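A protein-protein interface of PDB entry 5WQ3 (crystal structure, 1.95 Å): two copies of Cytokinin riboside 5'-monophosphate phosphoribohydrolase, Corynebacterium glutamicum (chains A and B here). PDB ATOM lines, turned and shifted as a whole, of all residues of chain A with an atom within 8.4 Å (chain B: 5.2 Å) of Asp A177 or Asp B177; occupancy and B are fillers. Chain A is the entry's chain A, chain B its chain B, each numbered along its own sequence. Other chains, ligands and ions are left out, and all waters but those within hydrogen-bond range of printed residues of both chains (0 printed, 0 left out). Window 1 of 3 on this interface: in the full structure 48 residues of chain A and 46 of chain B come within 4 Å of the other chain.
Among the printed residues, merely in contact across the chains: Phe A152 with Glu B181, Lys A156 with Lys B156, Phe A173 with Phe B180, Gly A174 with Cys B184, Leu A176 with Phe B180, Asp A177 with Phe B180, Asp A177 with Glu B181, Phe A180 with Phe B173, Phe A180 with Leu B176, Phe A180 with Asp B177, Phe A180 with Phe B180, Leu A183 with Phe B173 and Met A185 with Phe B152.
Hydrophobic or aromatic side chains of chain B that line the printed part of chain A: Phe B152, Phe B173, Leu B176 and Phe B180.
Along chain B the printed residues that touch a printed residue of chain A span positions 152 to 184.
Of the 22 printed residues of chain A, 11 touch a printed residue of chain B.
Among the printed residues, 19 pairs touch across the chains.
Among the printed residues, Asp or Glu carboxylates within 4 Å of a Lys or Arg side-chain nitrogen of the other chain: Lys A156 with Glu B181 (3.4 Å) and Glu A181 with Lys B156 (2.9 Å).
The side-chain amino group (NZ) of Lys A156 lies within salt-bridge range of the side-chain carboxylate (OD2) of Asp A177, 2.6 Å away.
OE1 of Glu A181 lies within salt-bridge range of NZ of Lys A156, at 2.6 Å.
The backbone carbonyl oxygen of Phe A180 is in hydrogen-bond range of the side-chain sulfur of Cys A184 (3.2 Å).
OD2 of Asp B177 is in salt-bridge range of NZ of Lys B156 (3.1 Å).
NZ of Lys B156 lies within salt-bridge range of OE2 of Glu B181 (2.7 Å).
The side-chain amino group (NZ) of Lys A156 is in salt-bridge range of the side-chain carboxylate (OE2) of Glu B181.
OE1 of Glu A181 lies within salt-bridge range of NZ of Lys B156, at 2.9 Å.
The backbone NH of Glu A181 lies within hydrogen-bond range of the side-chain carboxylate of Asp B177 (3.4 Å).
SG of Cys A184 is in hydrogen-bond range of O of Phe B173.
N of Gly B174 sits at hydrogen-bond distance from SG of Cys A184.
O of Asp A177 lies close to OD1 of Asp B177 (3.2 Å).
Phe A152 touches Glu B181, but with the chains exchanged Glu A181 does not touch Phe B152 (4.3 Å).
Lys A156 touches Glu B181, and with the chains exchanged Glu A181 touches Lys B156.
Gly A174 touches Cys B184, and with the chains exchanged Cys A184 touches Gly B174.
Asp A177 touches Glu B181, and with the chains exchanged Glu A181 touches Asp B177.
Of the 19 pairs that touch across the chains among the printed residues, 15 have their exchanged pair printed and touching as well.
Asp A177 touches just these residues of chain B: Asp B177, Phe B180 and Glu B181.
Of chain A, only Asp A177, Phe A180 and Glu A181 come within 4 Å of Asp B177.
Of the printed residues of chain A, Phe B180 touches Phe A173 (3.6 Å), Leu A176 (3.6 Å), Asp A177 (3.7 Å) and Phe A180 (3.8 Å).
Of the printed residues of chain B, Leu A183 touches Phe B173.
Printed residues of chain A within 4 Å of Cys B184: Gly A174 (3.98 Å).
The nearest printed residue of chain B that does not touch Asp A177 is Lys B156 (4.2 Å).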
ATOM      1  N   PHE A  74     -13.094   5.131  -5.058  1.00  0.00           N
ATOM      2  CA  PHE A  74     -12.885   6.019  -3.938  1.00  0.00           C
ATOM      3  C   PHE A  74     -14.168   6.493  -3.270  1.00  0.00           C
ATOM      4  O   PHE A  74     -15.272   6.427  -3.846  1.00  0.00           O
ATOM      5  CB  PHE A  74     -12.089   7.247  -4.380  1.00  0.00           C
ATOM      6  CG  PHE A  74     -10.639   7.145  -4.084  1.00  0.00           C
ATOM      7  CD1 PHE A  74      -9.866   6.181  -4.712  1.00  0.00           C
ATOM      8  CD2 PHE A  74     -10.044   7.997  -3.181  1.00  0.00           C
ATOM      9  CE1 PHE A  74      -8.517   6.077  -4.446  1.00  0.00           C
ATOM     10  CE2 PHE A  74      -8.686   7.904  -2.918  1.00  0.00           C
ATOM     11  CZ  PHE A  74      -7.928   6.932  -3.534  1.00  0.00           C
ATOM     12  N   PHE A 152       2.762   9.456  -0.900  1.00  0.00           N
ATOM     13  CA  PHE A 152       1.485   9.795  -1.491  1.00  0.00           C
ATOM     14  C   PHE A 152       1.536   9.738  -2.992  1.00  0.00           C
ATOM     15  O   PHE A 152       0.729   9.146  -3.608  1.00  0.00           O
ATOM     16  CB  PHE A 152       0.927  11.159  -0.984  1.00  0.00           C
ATOM     17  CG  PHE A 152       1.564  12.406  -1.622  1.00  0.00           C
ATOM     18  CD1 PHE A 152       2.731  12.975  -1.098  1.00  0.00           C
ATOM     19  CD2 PHE A 152       0.961  13.062  -2.715  1.00  0.00           C
ATOM     20  CE1 PHE A 152       3.274  14.111  -1.638  1.00  0.00           C
ATOM     21  CE2 PHE A 152       1.527  14.205  -3.274  1.00  0.00           C
ATOM     22  CZ  PHE A 152       2.693  14.718  -2.734  1.00  0.00           C
ATOM     23  N   ARG A 155       1.687   6.041  -4.280  1.00  0.00           N
ATOM     24  CA  ARG A 155       0.372   5.354  -4.184  1.00  0.00           C
ATOM     25  C   ARG A 155      -0.593   5.851  -5.310  1.00  0.00           C
ATOM     26  O   ARG A 155      -1.221   5.054  -6.000  1.00  0.00           O
ATOM     27  CB  ARG A 155      -0.171   5.551  -2.809  1.00  0.00           C
ATOM     28  CG  ARG A 155      -1.516   4.934  -2.502  1.00  0.00           C
ATOM     29  CD  ARG A 155      -2.314   5.986  -1.755  1.00  0.00           C
ATOM     30  NE  ARG A 155      -3.218   5.352  -0.859  1.00  0.00           N
ATOM     31  CZ  ARG A 155      -4.227   5.969  -0.292  1.00  0.00           C
ATOM     32  NH1 ARG A 155      -4.390   7.258  -0.514  1.00  0.00           N
ATOM     33  NH2 ARG A 155      -5.009   5.304   0.541  1.00  0.00           N
ATOM     34  N   LYS A 156      -0.640   7.161  -5.558  1.00  0.00           N
ATOM     35  CA  LYS A 156      -1.533   7.732  -6.624  1.00  0.00           C
ATOM     36  C   LYS A 156      -1.218   7.194  -7.961  1.00  0.00           C
ATOM     37  O   LYS A 156      -2.136   6.982  -8.800  1.00  0.00           O
ATOM     38  CB  LYS A 156      -1.433   9.220  -6.737  1.00  0.00           C
ATOM     39  CG  LYS A 156      -2.068   9.961  -5.577  1.00  0.00           C
ATOM     40  CD  LYS A 156      -1.543  11.395  -5.689  1.00  0.00           C
ATOM     41  CE  LYS A 156      -2.054  12.270  -4.578  1.00  0.00           C
ATOM     42  NZ  LYS A 156      -3.130  13.154  -5.034  1.00  0.00           N
ATOM     43  N   PHE A 166     -12.223   4.694 -12.886  1.00  0.00           N
ATOM     44  CA  PHE A 166     -12.445   5.249 -11.547  1.00  0.00           C
ATOM     45  C   PHE A 166     -13.964   5.395 -11.305  1.00  0.00           C
ATOM     46  O   PHE A 166     -14.671   5.925 -12.168  1.00  0.00           O
ATOM     47  CB  PHE A 166     -11.805   6.672 -11.458  1.00  0.00           C
ATOM     48  CG  PHE A 166     -10.325   6.708 -11.071  1.00  0.00           C
ATOM     49  CD1 PHE A 166      -9.510   5.582 -11.127  1.00  0.00           C
ATOM     50  CD2 PHE A 166      -9.746   7.913 -10.648  1.00  0.00           C
ATOM     51  CE1 PHE A 166      -8.163   5.644 -10.761  1.00  0.00           C
ATOM     52  CE2 PHE A 166      -8.415   7.980 -10.304  1.00  0.00           C
ATOM     53  CZ  PHE A 166      -7.629   6.835 -10.348  1.00  0.00           C
ATOM     54  N   CYS A 168     -16.246   7.183  -8.241  1.00  0.00           N
ATOM     55  CA  CYS A 168     -16.231   7.946  -7.002  1.00  0.00           C
ATOM     56  C   CYS A 168     -17.596   7.918  -6.294  1.00  0.00           C
ATOM     57  O   CYS A 168     -18.584   8.501  -6.730  1.00  0.00           O
ATOM     58  CB  CYS A 168     -15.772   9.375  -7.271  1.00  0.00           C
ATOM     59  SG  CYS A 168     -14.129   9.423  -8.026  1.00  0.00           S
ATOM     60  N   GLY A 171     -17.514  11.654  -1.220  1.00  0.00           N
ATOM     61  CA  GLY A 171     -16.369  11.828  -0.350  1.00  0.00           C
ATOM     62  C   GLY A 171     -15.951  13.257  -0.170  1.00  0.00           C
ATOM     63  O   GLY A 171     -16.546  14.203  -0.715  1.00  0.00           O
ATOM     64  N   GLY A 172     -14.916  13.391   0.634  1.00  0.00           N
ATOM     65  CA  GLY A 172     -14.341  14.631   0.969  1.00  0.00           C
ATOM     66  C   GLY A 172     -13.154  14.932   0.108  1.00  0.00           C
ATOM     67  O   GLY A 172     -13.134  14.626  -1.041  1.00  0.00           O
ATOM     68  N   PHE A 173     -12.170  15.551   0.701  1.00  0.00           N
ATOM     69  CA  PHE A 173     -11.058  16.157  -0.047  1.00  0.00           C
ATOM     70  C   PHE A 173     -10.178  15.132  -0.637  1.00  0.00           C
ATOM     71  O   PHE A 173      -9.726  15.305  -1.722  1.00  0.00           O
ATOM     72  CB  PHE A 173     -10.255  17.070   0.855  1.00  0.00           C
ATOM     73  CG  PHE A 173     -10.994  18.290   1.294  1.00  0.00           C
ATOM     74  CD1 PHE A 173     -12.038  18.812   0.550  1.00  0.00           C
ATOM     75  CD2 PHE A 173     -10.613  18.946   2.454  1.00  0.00           C
ATOM     76  CE1 PHE A 173     -12.700  19.949   0.981  1.00  0.00           C
ATOM     77  CE2 PHE A 173     -11.246  20.104   2.876  1.00  0.00           C
ATOM     78  CZ  PHE A 173     -12.286  20.613   2.146  1.00  0.00           C
ATOM     79  N   GLY A 174      -9.987  14.009   0.046  1.00  0.00           N
ATOM     80  CA  GLY A 174      -9.217  12.921  -0.525  1.00  0.00           C
ATOM     81  C   GLY A 174      -9.831  12.328  -1.759  1.00  0.00           C
ATOM     82  O   GLY A 174      -9.160  12.068  -2.772  1.00  0.00           O
ATOM     83  N   THR A 175     -11.134  12.127  -1.702  1.00  0.00           N
ATOM     84  CA  THR A 175     -11.880  11.716  -2.895  1.00  0.00           C
ATOM     85  C   THR A 175     -11.822  12.705  -4.007  1.00  0.00           C
ATOM     86  O   THR A 175     -11.572  12.344  -5.139  1.00  0.00           O
ATOM     87  CB  THR A 175     -13.339  11.488  -2.500  1.00  0.00           C
ATOM     88  OG1 THR A 175     -13.369  10.483  -1.469  1.00  0.00           O
ATOM     89  CG2 THR A 175     -14.092  10.992  -3.622  1.00  0.00           C
ATOM     90  N   LEU A 176     -11.993  13.984  -3.699  1.00  0.00           N
ATOM     91  CA  LEU A 176     -11.949  15.026  -4.724  1.00  0.00           C
ATOM     92  C   LEU A 176     -10.580  15.190  -5.363  1.00  0.00           C
ATOM     93  O   LEU A 176     -10.445  15.454  -6.560  1.00  0.00           O
ATOM     94  CB  LEU A 176     -12.397  16.386  -4.095  1.00  0.00           C
ATOM     95  CG  LEU A 176     -13.896  16.353  -3.576  1.00  0.00           C
ATOM     96  CD1 LEU A 176     -14.290  17.548  -2.771  1.00  0.00           C
ATOM     97  CD2 LEU A 176     -14.837  16.306  -4.742  1.00  0.00           C
ATOM     98  N   ASP A 177      -9.543  15.091  -4.552  1.00  0.00           N
ATOM     99  CA  ASP A 177      -8.124  15.065  -5.053  1.00  0.00           C
ATOM    100  C   ASP A 177      -7.955  14.013  -6.113  1.00  0.00           C
ATOM    101  O   ASP A 177      -7.353  14.250  -7.180  1.00  0.00           O
ATOM    102  CB  ASP A 177      -7.198  14.739  -3.861  1.00  0.00           C
ATOM    103  CG  ASP A 177      -5.721  14.717  -4.211  1.00  0.00           C
ATOM    104  OD1 ASP A 177      -5.345  15.284  -5.275  1.00  0.00           O
ATOM    105  OD2 ASP A 177      -4.964  14.108  -3.387  1.00  0.00           O
ATOM    106  N   GLU A 178      -8.450  12.809  -5.832  1.00  0.00           N
ATOM    107  CA  GLU A 178      -8.337  11.733  -6.869  1.00  0.00           C
ATOM    108  C   GLU A 178      -9.174  12.032  -8.065  1.00  0.00           C
ATOM    109  O   GLU A 178      -8.728  11.841  -9.187  1.00  0.00           O
ATOM    110  CB  GLU A 178      -8.728  10.345  -6.316  1.00  0.00           C
ATOM    111  CG  GLU A 178      -7.592   9.706  -5.578  1.00  0.00           C
ATOM    112  CD  GLU A 178      -6.442   9.174  -6.457  1.00  0.00           C
ATOM    113  OE1 GLU A 178      -6.596   8.776  -7.639  1.00  0.00           O
ATOM    114  OE2 GLU A 178      -5.348   9.066  -5.889  1.00  0.00           O
ATOM    115  N   LEU A 179     -10.420  12.457  -7.828  1.00  0.00           N
ATOM    116  CA  LEU A 179     -11.292  12.752  -8.970  1.00  0.00           C
ATOM    117  C   LEU A 179     -10.689  13.758  -9.892  1.00  0.00           C
ATOM    118  O   LEU A 179     -10.713  13.557 -11.077  1.00  0.00           O
ATOM    119  CB  LEU A 179     -12.639  13.247  -8.505  1.00  0.00           C
ATOM    120  CG  LEU A 179     -13.632  13.828  -9.553  1.00  0.00           C
ATOM    121  CD1 LEU A 179     -13.905  12.787 -10.592  1.00  0.00           C
ATOM    122  CD2 LEU A 179     -14.918  14.206  -8.863  1.00  0.00           C
ATOM    123  N   PHE A 180     -10.163  14.868  -9.389  1.00  0.00           N
ATOM    124  CA  PHE A 180      -9.603  15.889 -10.323  1.00  0.00           C
ATOM    125  C   PHE A 180      -8.303  15.527 -11.052  1.00  0.00           C
ATOM    126  O   PHE A 180      -8.073  15.925 -12.168  1.00  0.00           O
ATOM    127  CB  PHE A 180      -9.589  17.306  -9.653  1.00  0.00           C
ATOM    128  CG  PHE A 180     -11.008  17.874  -9.468  1.00  0.00           C
ATOM    129  CD1 PHE A 180     -11.763  18.229 -10.571  1.00  0.00           C
ATOM    130  CD2 PHE A 180     -11.609  17.925  -8.227  1.00  0.00           C
ATOM    131  CE1 PHE A 180     -13.064  18.663 -10.452  1.00  0.00           C
ATOM    132  CE2 PHE A 180     -12.921  18.357  -8.093  1.00  0.00           C
ATOM    133  CZ  PHE A 180     -13.646  18.719  -9.209  1.00  0.00           C
ATOM    134  N   GLU A 181      -7.467  14.739 -10.400  1.00  0.00           N
ATOM    135  CA  GLU A 181      -6.284  14.129 -10.971  1.00  0.00           C
ATOM    136  C   GLU A 181      -6.672  13.229 -12.171  1.00  0.00           C
ATOM    137  O   GLU A 181      -6.111  13.343 -13.256  1.00  0.00           O
ATOM    138  CB  GLU A 181      -5.724  13.256  -9.862  1.00  0.00           C
ATOM    139  CG  GLU A 181      -4.290  12.881  -9.856  1.00  0.00           C
ATOM    140  CD  GLU A 181      -3.962  12.377  -8.437  1.00  0.00           C
ATOM    141  OE1 GLU A 181      -4.027  13.233  -7.468  1.00  0.00           O
ATOM    142  OE2 GLU A 181      -3.725  11.127  -8.290  1.00  0.00           O
ATOM    143  N   VAL A 182      -7.632  12.336 -11.982  1.00  0.00           N
ATOM    144  CA  VAL A 182      -7.972  11.457 -13.095  1.00  0.00           C
ATOM    145  C   VAL A 182      -8.670  12.258 -14.211  1.00  0.00           C
ATOM    146  O   VAL A 182      -8.376  12.044 -15.375  1.00  0.00           O
ATOM    147  CB  VAL A 182      -8.757  10.210 -12.638  1.00  0.00           C
ATOM    148  CG1 VAL A 182     -10.190  10.555 -12.244  1.00  0.00           C
ATOM    149  CG2 VAL A 182      -8.694   9.141 -13.714  1.00  0.00           C
ATOM    150  N   LEU A 183      -9.524  13.227 -13.854  1.00  0.00           N
ATOM    151  CA  LEU A 183     -10.117  14.097 -14.882  1.00  0.00           C
ATOM    152  C   LEU A 183      -9.011  14.758 -15.670  1.00  0.00           C
ATOM    153  O   LEU A 183      -9.121  14.861 -16.905  1.00  0.00           O
ATOM    154  CB  LEU A 183     -11.110  15.100 -14.309  1.00  0.00           C
ATOM    155  CG  LEU A 183     -12.511  14.553 -13.945  1.00  0.00           C
ATOM    156  CD1 LEU A 183     -13.247  15.471 -12.984  1.00  0.00           C
ATOM    157  CD2 LEU A 183     -13.305  14.395 -15.237  1.00  0.00           C
ATOM    158  N   CYS A 184      -7.927  15.179 -15.006  1.00  0.00           N
ATOM    159  CA  CYS A 184      -6.779  15.782 -15.752  1.00  0.00           C
ATOM    160  C   CYS A 184      -6.064  14.790 -16.670  1.00  0.00           C
ATOM    161  O   CYS A 184      -5.636  15.128 -17.774  1.00  0.00           O
ATOM    162  CB  CYS A 184      -5.685  16.317 -14.819  1.00  0.00           C
ATOM    163  SG  CYS A 184      -6.051  17.742 -13.797  1.00  0.00           S
ATOM    164  N   MET A 185      -5.832  13.587 -16.159  1.00  0.00           N
ATOM    165  CA  MET A 185      -5.102  12.559 -16.919  1.00  0.00           C
ATOM    166  C   MET A 185      -5.854  12.156 -18.213  1.00  0.00           C
ATOM    167  O   MET A 185      -5.264  11.895 -19.279  1.00  0.00           O
ATOM    168  CB  MET A 185      -4.855  11.361 -15.988  1.00  0.00           C
ATOM    169  CG  MET A 185      -3.899  11.666 -14.813  1.00  0.00           C
ATOM    170  SD  MET A 185      -2.166  11.794 -15.294  1.00  0.00           S
ATOM    171  CE  MET A 185      -1.982  13.502 -15.763  1.00  0.00           C
ATOM    172  N   TRP A 204     -23.607  14.933  -5.911  1.00  0.00           N
ATOM    173  CA  TRP A 204     -22.606  15.483  -6.852  1.00  0.00           C
ATOM    174  C   TRP A 204     -23.123  16.662  -7.662  1.00  0.00           C
ATOM    175  O   TRP A 204     -22.344  17.496  -8.196  1.00  0.00           O
ATOM    176  CB  TRP A 204     -22.099  14.384  -7.779  1.00  0.00           C
ATOM    177  CG  TRP A 204     -21.206  13.352  -7.082  1.00  0.00           C
ATOM    178  CD1 TRP A 204     -21.535  12.061  -6.734  1.00  0.00           C
ATOM    179  CD2 TRP A 204     -19.833  13.524  -6.707  1.00  0.00           C
ATOM    180  NE1 TRP A 204     -20.470  11.445  -6.116  1.00  0.00           N
ATOM    181  CE2 TRP A 204     -19.408  12.312  -6.092  1.00  0.00           C
ATOM    182  CE3 TRP A 204     -18.912  14.576  -6.835  1.00  0.00           C
ATOM    183  CZ2 TRP A 204     -18.091  12.126  -5.612  1.00  0.00           C
ATOM    184  CZ3 TRP A 204     -17.633  14.412  -6.313  1.00  0.00           C
ATOM    185  CH2 TRP A 204     -17.230  13.181  -5.707  1.00  0.00           C
ATOM    186  N   PHE B 152       3.833  13.902 -14.177  1.00  0.00           N
ATOM    187  CA  PHE B 152       2.850  14.591 -13.396  1.00  0.00           C
ATOM    188  C   PHE B 152       3.055  14.543 -11.888  1.00  0.00           C
ATOM    189  O   PHE B 152       3.099  15.549 -11.247  1.00  0.00           O
ATOM    190  CB  PHE B 152       1.517  13.956 -13.723  1.00  0.00           C
ATOM    191  CG  PHE B 152       0.386  14.823 -13.479  1.00  0.00           C
ATOM    192  CD1 PHE B 152       0.272  15.992 -14.144  1.00  0.00           C
ATOM    193  CD2 PHE B 152      -0.594  14.461 -12.585  1.00  0.00           C
ATOM    194  CE1 PHE B 152      -0.800  16.805 -13.902  1.00  0.00           C
ATOM    195  CE2 PHE B 152      -1.665  15.258 -12.344  1.00  0.00           C
ATOM    196  CZ  PHE B 152      -1.768  16.433 -12.995  1.00  0.00           C
ATOM    197  N   LYS B 156       4.148  17.621  -9.099  1.00  0.00           N
ATOM    198  CA  LYS B 156       3.274  17.951  -7.995  1.00  0.00           C
ATOM    199  C   LYS B 156       3.932  17.942  -6.651  1.00  0.00           C
ATOM    200  O   LYS B 156       3.685  18.779  -5.860  1.00  0.00           O
ATOM    201  CB  LYS B 156       2.082  17.025  -7.965  1.00  0.00           C
ATOM    202  CG  LYS B 156       0.978  17.442  -8.886  1.00  0.00           C
ATOM    203  CD  LYS B 156      -0.374  17.166  -8.268  1.00  0.00           C
ATOM    204  CE  LYS B 156      -1.003  15.913  -8.827  1.00  0.00           C
ATOM    205  NZ  LYS B 156      -2.043  15.353  -7.927  1.00  0.00           N
ATOM    206  N   GLY B 172      -9.068  25.415 -14.163  1.00  0.00           N
ATOM    207  CA  GLY B 172      -9.810  24.236 -14.517  1.00  0.00           C
ATOM    208  C   GLY B 172      -9.374  23.091 -13.650  1.00  0.00           C
ATOM    209  O   GLY B 172      -9.115  23.275 -12.454  1.00  0.00           O
ATOM    210  N   PHE B 173      -9.281  21.908 -14.234  1.00  0.00           N
ATOM    211  CA  PHE B 173      -9.131  20.696 -13.439  1.00  0.00           C
ATOM    212  C   PHE B 173      -7.748  20.550 -12.842  1.00  0.00           C
ATOM    213  O   PHE B 173      -7.599  19.977 -11.762  1.00  0.00           O
ATOM    214  CB  PHE B 173      -9.470  19.463 -14.285  1.00  0.00           C
ATOM    215  CG  PHE B 173     -10.940  19.341 -14.676  1.00  0.00           C
ATOM    216  CD1 PHE B 173     -11.946  19.849 -13.880  1.00  0.00           C
ATOM    217  CD2 PHE B 173     -11.302  18.580 -15.786  1.00  0.00           C
ATOM    218  CE1 PHE B 173     -13.283  19.660 -14.184  1.00  0.00           C
ATOM    219  CE2 PHE B 173     -12.633  18.416 -16.125  1.00  0.00           C
ATOM    220  CZ  PHE B 173     -13.622  18.937 -15.306  1.00  0.00           C
ATOM    221  N   GLY B 174      -6.733  21.045 -13.543  1.00  0.00           N
ATOM    222  CA  GLY B 174      -5.390  21.034 -13.011  1.00  0.00           C
ATOM    223  C   GLY B 174      -5.258  21.889 -11.745  1.00  0.00           C
ATOM    224  O   GLY B 174      -4.573  21.501 -10.792  1.00  0.00           O
ATOM    225  N   THR B 175      -5.965  23.021 -11.715  1.00  0.00           N
ATOM    226  CA  THR B 175      -5.969  23.886 -10.527  1.00  0.00           C
ATOM    227  C   THR B 175      -6.728  23.219  -9.426  1.00  0.00           C
ATOM    228  O   THR B 175      -6.269  23.174  -8.296  1.00  0.00           O
ATOM    229  CB  THR B 175      -6.569  25.273 -10.821  1.00  0.00           C
ATOM    230  OG1 THR B 175      -5.729  25.960 -11.768  1.00  0.00           O
ATOM    231  CG2 THR B 175      -6.702  26.097  -9.528  1.00  0.00           C
ATOM    232  N   LEU B 176      -7.905  22.695  -9.753  1.00  0.00           N
ATOM    233  CA  LEU B 176      -8.745  22.024  -8.767  1.00  0.00           C
ATOM    234  C   LEU B 176      -8.024  20.836  -8.139  1.00  0.00           C
ATOM    235  O   LEU B 176      -8.126  20.600  -6.936  1.00  0.00           O
ATOM    236  CB  LEU B 176     -10.057  21.564  -9.407  1.00  0.00           C
ATOM    237  CG  LEU B 176     -11.060  22.664  -9.760  1.00  0.00           C
ATOM    238  CD1 LEU B 176     -12.191  22.106 -10.611  1.00  0.00           C
ATOM    239  CD2 LEU B 176     -11.605  23.320  -8.501  1.00  0.00           C
ATOM    240  N   ASP B 177      -7.295  20.089  -8.963  1.00  0.00           N
ATOM    241  CA  ASP B 177      -6.562  18.921  -8.491  1.00  0.00           C
ATOM    242  C   ASP B 177      -5.529  19.303  -7.437  1.00  0.00           C
ATOM    243  O   ASP B 177      -5.339  18.588  -6.452  1.00  0.00           O
ATOM    244  CB  ASP B 177      -5.879  18.208  -9.661  1.00  0.00           C
ATOM    245  CG  ASP B 177      -4.925  17.122  -9.205  1.00  0.00           C
ATOM    246  OD1 ASP B 177      -5.287  16.358  -8.286  1.00  0.00           O
ATOM    247  OD2 ASP B 177      -3.812  17.032  -9.766  1.00  0.00           O
ATOM    248  N   GLU B 178      -4.863  20.434  -7.648  1.00  0.00           N
ATOM    249  CA  GLU B 178      -3.845  20.909  -6.719  1.00  0.00           C
ATOM    250  C   GLU B 178      -4.472  21.443  -5.435  1.00  0.00           C
ATOM    251  O   GLU B 178      -3.925  21.267  -4.346  1.00  0.00           O
ATOM    252  CB  GLU B 178      -2.985  21.991  -7.374  1.00  0.00           C
ATOM    253  CG  GLU B 178      -1.930  21.453  -8.326  1.00  0.00           C
ATOM    254  CD  GLU B 178      -0.747  20.842  -7.599  1.00  0.00           C
ATOM    255  OE1 GLU B 178       0.165  20.324  -8.276  1.00  0.00           O
ATOM    256  OE2 GLU B 178      -0.731  20.880  -6.351  1.00  0.00           O
ATOM    257  N   LEU B 179      -5.621  22.097  -5.571  1.00  0.00           N
ATOM    258  CA  LEU B 179      -6.310  22.656  -4.439  1.00  0.00           C
ATOM    259  C   LEU B 179      -6.772  21.543  -3.473  1.00  0.00           C
ATOM    260  O   LEU B 179      -6.629  21.667  -2.259  1.00  0.00           O
ATOM    261  CB  LEU B 179      -7.511  23.520  -4.904  1.00  0.00           C
ATOM    262  CG  LEU B 179      -8.562  23.857  -3.862  1.00  0.00           C
ATOM    263  CD1 LEU B 179      -7.879  24.749  -2.804  1.00  0.00           C
ATOM    264  CD2 LEU B 179      -9.812  24.516  -4.489  1.00  0.00           C
ATOM    265  N   PHE B 180      -7.374  20.485  -4.004  1.00  0.00           N
ATOM    266  CA  PHE B 180      -7.858  19.461  -3.087  1.00  0.00           C
ATOM    267  C   PHE B 180      -6.718  18.560  -2.518  1.00  0.00           C
ATOM    268  O   PHE B 180      -6.840  18.040  -1.435  1.00  0.00           O
ATOM    269  CB  PHE B 180      -8.952  18.647  -3.752  1.00  0.00           C
ATOM    270  CG  PHE B 180     -10.255  19.403  -3.853  1.00  0.00           C
ATOM    271  CD1 PHE B 180     -10.945  19.735  -2.713  1.00  0.00           C
ATOM    272  CD2 PHE B 180     -10.740  19.811  -5.077  1.00  0.00           C
ATOM    273  CE1 PHE B 180     -12.140  20.434  -2.786  1.00  0.00           C
ATOM    274  CE2 PHE B 180     -11.916  20.516  -5.167  1.00  0.00           C
ATOM    275  CZ  PHE B 180     -12.619  20.839  -4.018  1.00  0.00           C
ATOM    276  N   GLU B 181      -5.629  18.403  -3.257  1.00  0.00           N
ATOM    277  CA  GLU B 181      -4.417  17.801  -2.719  1.00  0.00           C
ATOM    278  C   GLU B 181      -3.902  18.539  -1.506  1.00  0.00           C
ATOM    279  O   GLU B 181      -3.716  17.921  -0.462  1.00  0.00           O
ATOM    280  CB  GLU B 181      -3.372  17.686  -3.780  1.00  0.00           C
ATOM    281  CG  GLU B 181      -2.113  17.010  -3.329  1.00  0.00           C
ATOM    282  CD  GLU B 181      -1.135  16.885  -4.487  1.00  0.00           C
ATOM    283  OE1 GLU B 181      -0.122  17.610  -4.468  1.00  0.00           O
ATOM    284  OE2 GLU B 181      -1.411  16.091  -5.425  1.00  0.00           O
ATOM    285  N   CYS B 184      -6.238  18.324   1.513  1.00  0.00           N
ATOM    286  CA  CYS B 184      -6.125  17.008   2.145  1.00  0.00           C
ATOM    287  C   CYS B 184      -4.802  16.804   2.928  1.00  0.00           C
ATOM    288  O   CYS B 184      -4.762  16.049   3.897  1.00  0.00           O
ATOM    289  CB  CYS B 184      -6.301  15.912   1.086  1.00  0.00           C
ATOM    290  SG  CYS B 184      -6.197  14.224   1.721  1.00  0.00           S
